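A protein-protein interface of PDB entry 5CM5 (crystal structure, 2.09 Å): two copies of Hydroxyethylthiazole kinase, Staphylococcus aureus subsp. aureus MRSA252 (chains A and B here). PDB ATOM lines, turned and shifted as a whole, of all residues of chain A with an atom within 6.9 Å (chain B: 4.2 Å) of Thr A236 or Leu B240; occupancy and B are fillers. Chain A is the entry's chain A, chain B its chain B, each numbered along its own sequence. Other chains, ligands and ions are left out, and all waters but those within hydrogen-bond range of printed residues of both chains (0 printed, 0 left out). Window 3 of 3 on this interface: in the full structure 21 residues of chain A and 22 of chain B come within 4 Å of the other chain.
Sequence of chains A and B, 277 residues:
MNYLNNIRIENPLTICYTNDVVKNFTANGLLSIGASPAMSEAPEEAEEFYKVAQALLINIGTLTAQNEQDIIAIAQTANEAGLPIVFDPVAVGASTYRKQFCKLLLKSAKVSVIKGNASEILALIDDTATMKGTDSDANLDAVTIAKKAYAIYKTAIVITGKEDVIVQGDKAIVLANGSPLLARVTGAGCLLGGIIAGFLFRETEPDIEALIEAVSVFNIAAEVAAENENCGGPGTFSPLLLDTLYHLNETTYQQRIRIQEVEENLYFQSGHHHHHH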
ATOM      1  N   ALA A 225     -31.500  -8.632  -2.789  1.00  0.00           N
ATOM      2  CA  ALA A 225     -30.059  -8.840  -2.962  1.00  0.00           C
ATOM      3  C   ALA A 225     -29.248  -8.048  -1.904  1.00  0.00           C
ATOM      4  O   ALA A 225     -28.297  -8.569  -1.304  1.00  0.00           O
ATOM      5  CB  ALA A 225     -29.601  -8.457  -4.356  1.00  0.00           C
ATOM      6  N   ASN A 230     -24.231 -12.034   2.430  1.00  0.00           N
ATOM      7  CA  ASN A 230     -22.985 -11.982   1.650  1.00  0.00           C
ATOM      8  C   ASN A 230     -22.859 -10.728   0.790  1.00  0.00           C
ATOM      9  O   ASN A 230     -21.912 -10.618   0.002  1.00  0.00           O
ATOM     10  CB  ASN A 230     -22.857 -13.230   0.741  1.00  0.00           C
ATOM     11  CG  ASN A 230     -22.994 -14.542   1.547  1.00  0.00           C
ATOM     12  OD1 ASN A 230     -22.247 -14.775   2.467  1.00  0.00           O
ATOM     13  ND2 ASN A 230     -24.051 -15.295   1.265  1.00  0.00           N
ATOM     14  N   CYS A 231     -23.790  -9.795   0.942  1.00  0.00           N
ATOM     15  CA  CYS A 231     -23.652  -8.494   0.220  1.00  0.00           C
ATOM     16  C   CYS A 231     -22.794  -7.582   1.067  1.00  0.00           C
ATOM     17  O   CYS A 231     -23.275  -7.043   2.065  1.00  0.00           O
ATOM     18  CB  CYS A 231     -24.980  -7.852   0.031  1.00  0.00           C
ATOM     19  SG  CYS A 231     -24.905  -6.360  -1.019  1.00  0.00           S
ATOM     20  N   GLY A 232     -21.541  -7.416   0.700  1.00  0.00           N
ATOM     21  CA  GLY A 232     -20.643  -6.558   1.438  1.00  0.00           C
ATOM     22  C   GLY A 232     -20.427  -5.180   0.832  1.00  0.00           C
ATOM     23  O   GLY A 232     -19.560  -4.444   1.276  1.00  0.00           O
ATOM     24  N   GLY A 233     -21.153  -4.851  -0.221  1.00  0.00           N
ATOM     25  CA  GLY A 233     -20.877  -3.608  -0.917  1.00  0.00           C
ATOM     26  C   GLY A 233     -21.309  -3.679  -2.361  1.00  0.00           C
ATOM     27  O   GLY A 233     -21.934  -4.649  -2.800  1.00  0.00           O
ATOM     28  N   PRO A 234     -21.065  -2.606  -3.118  1.00  0.00           N
ATOM     29  CA  PRO A 234     -21.524  -2.569  -4.522  1.00  0.00           C
ATOM     30  C   PRO A 234     -20.901  -3.627  -5.467  1.00  0.00           C
ATOM     31  O   PRO A 234     -21.524  -4.039  -6.439  1.00  0.00           O
ATOM     32  CB  PRO A 234     -21.120  -1.161  -4.997  1.00  0.00           C
ATOM     33  CG  PRO A 234     -20.051  -0.732  -4.091  1.00  0.00           C
ATOM     34  CD  PRO A 234     -20.273  -1.436  -2.757  1.00  0.00           C
ATOM     35  N   GLY A 235     -19.697  -4.106  -5.122  1.00  0.00           N
ATOM     36  CA  GLY A 235     -19.091  -5.198  -5.875  1.00  0.00           C
ATOM     37  C   GLY A 235     -19.880  -6.481  -5.745  1.00  0.00           C
ATOM     38  O   GLY A 235     -20.243  -7.100  -6.729  1.00  0.00           O
ATOM     39  N   THR A 236     -19.998  -6.983  -4.514  1.00  0.00           N
ATOM     40  CA  THR A 236     -20.694  -8.249  -4.306  1.00  0.00           C
ATOM     41  C   THR A 236     -22.198  -8.180  -4.572  1.00  0.00           C
ATOM     42  O   THR A 236     -22.856  -9.179  -4.906  1.00  0.00           O
ATOM     43  CB  THR A 236     -20.429  -8.818  -2.909  1.00  0.00           C
ATOM     44  OG1 THR A 236     -20.577  -7.800  -1.910  1.00  0.00           O
ATOM     45  CG2 THR A 236     -18.984  -9.372  -2.842  1.00  0.00           C
ATOM     46  N   PHE A 237     -22.758  -6.989  -4.434  1.00  0.00           N
ATOM     47  CA  PHE A 237     -24.163  -6.794  -4.760  1.00  0.00           C
ATOM     48  C   PHE A 237     -24.549  -7.281  -6.154  1.00  0.00           C
ATOM     49  O   PHE A 237     -25.620  -7.849  -6.379  1.00  0.00           O
ATOM     50  CB  PHE A 237     -24.529  -5.297  -4.574  1.00  0.00           C
ATOM     51  CG  PHE A 237     -25.890  -4.931  -5.083  1.00  0.00           C
ATOM     52  CD1 PHE A 237     -27.009  -5.161  -4.330  1.00  0.00           C
ATOM     53  CD2 PHE A 237     -26.032  -4.295  -6.283  1.00  0.00           C
ATOM     54  CE1 PHE A 237     -28.268  -4.755  -4.774  1.00  0.00           C
ATOM     55  CE2 PHE A 237     -27.295  -3.883  -6.771  1.00  0.00           C
ATOM     56  CZ  PHE A 237     -28.414  -4.165  -6.024  1.00  0.00           C
ATOM     57  N   SER A 238     -23.726  -6.973  -7.121  1.00  0.00           N
ATOM     58  CA  SER A 238     -24.122  -7.151  -8.517  1.00  0.00           C
ATOM     59  C   SER A 238     -24.344  -8.648  -8.843  1.00  0.00           C
ATOM     60  O   SER A 238     -25.402  -8.989  -9.364  1.00  0.00           O
ATOM     61  CB  SER A 238     -23.164  -6.416  -9.441  1.00  0.00           C
ATOM     62  OG  SER A 238     -23.419  -6.745 -10.790  1.00  0.00           O
ATOM     63  N   PRO A 239     -23.408  -9.554  -8.501  1.00  0.00           N
ATOM     64  CA  PRO A 239     -23.731 -10.969  -8.719  1.00  0.00           C
ATOM     65  C   PRO A 239     -24.964 -11.416  -7.978  1.00  0.00           C
ATOM     66  O   PRO A 239     -25.739 -12.274  -8.470  1.00  0.00           O
ATOM     67  CB  PRO A 239     -22.499 -11.681  -8.161  1.00  0.00           C
ATOM     68  CG  PRO A 239     -21.389 -10.724  -8.437  1.00  0.00           C
ATOM     69  CD  PRO A 239     -21.987  -9.360  -8.170  1.00  0.00           C
ATOM     70  N   LEU A 240     -25.201 -10.835  -6.808  1.00  0.00           N
ATOM     71  CA  LEU A 240     -26.362 -11.221  -6.002  1.00  0.00           C
ATOM     72  C   LEU A 240     -27.647 -10.688  -6.643  1.00  0.00           C
ATOM     73  O   LEU A 240     -28.706 -11.336  -6.553  1.00  0.00           O
ATOM     74  CB  LEU A 240     -26.192 -10.758  -4.582  1.00  0.00           C
ATOM     75  CG  LEU A 240     -25.054 -11.444  -3.800  1.00  0.00           C
ATOM     76  CD1 LEU A 240     -24.739 -10.660  -2.531  1.00  0.00           C
ATOM     77  CD2 LEU A 240     -25.363 -12.891  -3.484  1.00  0.00           C
ATOM     78  N   LEU A 241     -27.597  -9.520  -7.227  1.00  0.00           N
ATOM     79  CA  LEU A 241     -28.765  -9.037  -7.971  1.00  0.00           C
ATOM     80  C   LEU A 241     -29.168 -10.030  -9.042  1.00  0.00           C
ATOM     81  O   LEU A 241     -30.338 -10.362  -9.213  1.00  0.00           O
ATOM     82  CB  LEU A 241     -28.438  -7.678  -8.566  1.00  0.00           C
ATOM     83  CG  LEU A 241     -29.490  -7.075  -9.482  1.00  0.00           C
ATOM     84  CD1 LEU A 241     -30.802  -6.851  -8.747  1.00  0.00           C
ATOM     85  CD2 LEU A 241     -29.031  -5.718 -10.027  1.00  0.00           C
ATOM     86  N   ALA B 225      -8.740  -6.679   0.134  1.00  0.00           N
ATOM     87  CA  ALA B 225      -9.643  -7.579  -0.605  1.00  0.00           C
ATOM     88  C   ALA B 225      -9.082  -9.012  -0.724  1.00  0.00           C
ATOM     89  O   ALA B 225      -9.808  -9.962  -0.533  1.00  0.00           O
ATOM     90  CB  ALA B 225      -9.950  -7.042  -1.998  1.00  0.00           C
ATOM     91  N   ASN B 230     -13.558 -14.614   1.897  1.00  0.00           N
ATOM     92  CA  ASN B 230     -14.348 -15.042   0.738  1.00  0.00           C
ATOM     93  C   ASN B 230     -13.635 -14.858  -0.588  1.00  0.00           C
ATOM     94  O   ASN B 230     -14.231 -15.070  -1.632  1.00  0.00           O
ATOM     95  CB  ASN B 230     -15.713 -14.322   0.724  1.00  0.00           C
ATOM     96  CG  ASN B 230     -16.444 -14.430   2.065  1.00  0.00           C
ATOM     97  OD1 ASN B 230     -16.812 -15.539   2.499  1.00  0.00           O
ATOM     98  ND2 ASN B 230     -16.637 -13.290   2.740  1.00  0.00           N
ATOM     99  N   CYS B 231     -12.367 -14.450  -0.560  1.00  0.00           N
ATOM    100  CA  CYS B 231     -11.593 -14.339  -1.785  1.00  0.00           C
ATOM    101  C   CYS B 231     -10.966 -15.666  -2.144  1.00  0.00           C
ATOM    102  O   CYS B 231     -10.038 -16.094  -1.486  1.00  0.00           O
ATOM    103  CB  CYS B 231     -10.469 -13.356  -1.624  1.00  0.00           C
ATOM    104  SG  CYS B 231      -9.592 -13.004  -3.197  1.00  0.00           S
ATOM    105  N   THR B 236     -13.562 -14.058  -7.599  1.00  0.00           N
ATOM    106  CA  THR B 236     -14.164 -13.452  -6.426  1.00  0.00           C
ATOM    107  C   THR B 236     -13.401 -12.232  -5.919  1.00  0.00           C
ATOM    108  O   THR B 236     -14.030 -11.349  -5.296  1.00  0.00           O
ATOM    109  CB  THR B 236     -14.331 -14.501  -5.310  1.00  0.00           C
ATOM    110  OG1 THR B 236     -13.106 -15.219  -5.131  1.00  0.00           O
ATOM    111  CG2 THR B 236     -15.436 -15.455  -5.705  1.00  0.00           C
ATOM    112  N   PHE B 237     -12.116 -12.097  -6.237  1.00  0.00           N
ATOM    113  CA  PHE B 237     -11.338 -10.937  -5.828  1.00  0.00           C
ATOM    114  C   PHE B 237     -11.941  -9.572  -6.399  1.00  0.00           C
ATOM    115  O   PHE B 237     -12.044  -8.599  -5.689  1.00  0.00           O
ATOM    116  CB  PHE B 237      -9.905 -11.105  -6.356  1.00  0.00           C
ATOM    117  CG  PHE B 237      -9.045  -9.867  -6.258  1.00  0.00           C
ATOM    118  CD1 PHE B 237      -8.462  -9.511  -5.066  1.00  0.00           C
ATOM    119  CD2 PHE B 237      -8.899  -9.008  -7.344  1.00  0.00           C
ATOM    120  CE1 PHE B 237      -7.714  -8.354  -4.947  1.00  0.00           C
ATOM    121  CE2 PHE B 237      -8.135  -7.828  -7.235  1.00  0.00           C
ATOM    122  CZ  PHE B 237      -7.585  -7.472  -6.013  1.00  0.00           C
ATOM    123  N   SER B 238     -12.391  -9.606  -7.627  1.00  0.00           N
ATOM    124  CA  SER B 238     -12.835  -8.350  -8.283  1.00  0.00           C
ATOM    125  C   SER B 238     -14.041  -7.680  -7.587  1.00  0.00           C
ATOM    126  O   SER B 238     -13.944  -6.529  -7.176  1.00  0.00           O
ATOM    127  CB  SER B 238     -13.003  -8.567  -9.778  1.00  0.00           C
ATOM    128  OG  SER B 238     -13.583  -7.391 -10.309  1.00  0.00           O
ATOM    129  N   PRO B 239     -15.180  -8.381  -7.415  1.00  0.00           N
ATOM    130  CA  PRO B 239     -16.172  -7.781  -6.537  1.00  0.00           C
ATOM    131  C   PRO B 239     -15.717  -7.305  -5.149  1.00  0.00           C
ATOM    132  O   PRO B 239     -16.217  -6.310  -4.623  1.00  0.00           O
ATOM    133  CB  PRO B 239     -17.212  -8.907  -6.366  1.00  0.00           C
ATOM    134  CG  PRO B 239     -17.076  -9.685  -7.665  1.00  0.00           C
ATOM    135  CD  PRO B 239     -15.601  -9.700  -7.910  1.00  0.00           C
ATOM    136  N   LEU B 240     -14.863  -8.096  -4.493  1.00  0.00           N
ATOM    137  CA  LEU B 240     -14.375  -7.710  -3.220  1.00  0.00           C
ATOM    138  C   LEU B 240     -13.483  -6.481  -3.267  1.00  0.00           C
ATOM    139  O   LEU B 240     -13.442  -5.683  -2.330  1.00  0.00           O
ATOM    140  CB  LEU B 240     -13.609  -8.902  -2.584  1.00  0.00           C
ATOM    141  CG  LEU B 240     -14.495 -10.099  -2.280  1.00  0.00           C
ATOM    142  CD1 LEU B 240     -13.646 -11.349  -1.939  1.00  0.00           C
ATOM    143  CD2 LEU B 240     -15.455  -9.832  -1.121  1.00  0.00           C
ATOM    144  N   LEU B 241     -12.703  -6.342  -4.303  1.00  0.00           N
ATOM    145  CA  LEU B 241     -11.916  -5.121  -4.498  1.00  0.00           C
ATOM    146  C   LEU B 241     -12.854  -3.880  -4.524  1.00  0.00           C
ATOM    147  O   LEU B 241     -12.621  -2.880  -3.850  1.00  0.00           O
ATOM    148  CB  LEU B 241     -11.137  -5.171  -5.827  1.00  0.00           C
ATOM    149  CG  LEU B 241     -10.396  -3.895  -6.238  1.00  0.00           C
ATOM    150  CD1 LEU B 241      -9.354  -3.492  -5.205  1.00  0.00           C
ATOM    151  CD2 LEU B 241      -9.699  -4.078  -7.577  1.00  0.00           C
ATOM    152  N   LEU B 242     -13.964  -4.018  -5.202  1.00  0.00           N
ATOM    153  CA  LEU B 242     -14.944  -2.884  -5.289  1.00  0.00           C
ATOM    154  C   LEU B 242     -15.581  -2.633  -3.912  1.00  0.00           C
ATOM    155  O   LEU B 242     -15.777  -1.478  -3.530  1.00  0.00           O
ATOM    156  CB  LEU B 242     -15.988  -3.174  -6.297  1.00  0.00           C
ATOM    157  CG  LEU B 242     -15.525  -3.219  -7.747  1.00  0.00           C
ATOM    158  CD1 LEU B 242     -16.640  -3.704  -8.701  1.00  0.00           C
ATOM    159  CD2 LEU B 242     -14.995  -1.896  -8.250  1.00  0.00           C
ATOM    160  N   ASP B 243     -15.898  -3.711  -3.177  1.00  0.00           N
ATOM    161  CA  ASP B 243     -16.469  -3.528  -1.866  1.00  0.00           C
ATOM    162  C   ASP B 243     -15.486  -2.756  -0.988  1.00  0.00           C
ATOM    163  O   ASP B 243     -15.901  -1.942  -0.183  1.00  0.00           O
ATOM    164  CB  ASP B 243     -16.782  -4.907  -1.157  1.00  0.00           C
ATOM    165  CG  ASP B 243     -18.018  -5.589  -1.736  1.00  0.00           C
ATOM    166  OD1 ASP B 243     -18.647  -5.014  -2.693  1.00  0.00           O
ATOM    167  OD2 ASP B 243     -18.364  -6.661  -1.323  1.00  0.00           O
ATOM    168  N   THR B 244     -14.205  -3.154  -1.075  1.00  0.00           N
ATOM    169  CA  THR B 244     -13.175  -2.680  -0.172  1.00  0.00           C
ATOM    170  C   THR B 244     -12.859  -1.220  -0.473  1.00  0.00           C
ATOM    171  O   THR B 244     -12.671  -0.430   0.458  1.00  0.00           O
ATOM    172  CB  THR B 244     -11.902  -3.503  -0.302  1.00  0.00           C
ATOM    173  OG1 THR B 244     -12.185  -4.894  -0.035  1.00  0.00           O
ATOM    174  CG2 THR B 244     -10.888  -3.018   0.659  1.00  0.00           C
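Hydrophobic or aromatic side chains of chain A within 4 Å of the printed part of chain B: Pro A234. Of the 12 printed residues of chain B, 4 touch a printed residue of chain A. Printed residues of chain B that touch a printed residue of chain A: Pro B239, Leu B240, Leu B242 and Asp B243. Hydrophobic or aromatic side chains of chain B that line the printed part of chain A: Pro B239, Leu B240 and Leu B242.
Printed residues of chain B within 4 Å of Gly A232: Asp B243. Printed residues of chain B within 4 Å of Gly A233: Asp B243 (3.0 Å). Of the printed residues of chain B, Pro A234 touches Asp B243 (3.4 Å). Thr A236 touches just these residues of chain B: Pro B239 (3.8 Å), Leu B240 (3.95 Å) and Asp B243 (2.6 Å). Ala B225 touches none of the printed residues of chain A. Leu B240 touches just one residue of chain A: Thr A236. Of the printed residues of chain A, Leu B242 touches Gly A235 (3.7 Å). Thr B244 touches none of the printed residues of chain A. The nearest residue of chain A that does not touch Leu B240 is Gly A235 (5.3 Å).
N of Gly A235 is in hydrogen-bond range of OD1 of Asp B243. OG1 of Thr A236 sits at hydrogen-bond distance from OD2 of Asp B243, at 2.6 Å. The side-chain carboxylate (OD1) of Asp B243 lies close to the backbone carbonyl oxygen (O) of Gly A233 (3.3 Å). N of Pro A234 sits close to OD1 of Asp B243, at 3.4 Å.
Thr A236 touches Pro B239, but with the chains exchanged Pro A239 does not touch Thr B236 (8.0 Å). Thr A236 touches Leu B240, but with the chains exchanged Leu A240 does not touch Thr B236 (10.5 Å). Positions printed for both chains: 225, 230, 231, 236, 237, 238, 239, 240 and 241.
Among the printed residues, pairs that only touch across the chains: Gly A235 with Pro B239 (3.3 Å), Gly A232 with Asp B243 (3.3 Å), Gly A235 with Leu B242 (3.7 Å), Thr A236 with Pro B239 (3.8 Å) and Thr A236 with Leu B240 (3.95 Å).
OG1 of Thr A236 is in hydrogen-bond range of N of Gly A232 (2.8 Å). N of Gly A233 lies within hydrogen-bond range of OG1 of Thr A236, at 3.4 Å. O of Leu B240 lies within hydrogen-bond range of OG1 of Thr B244 (2.7 Å).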
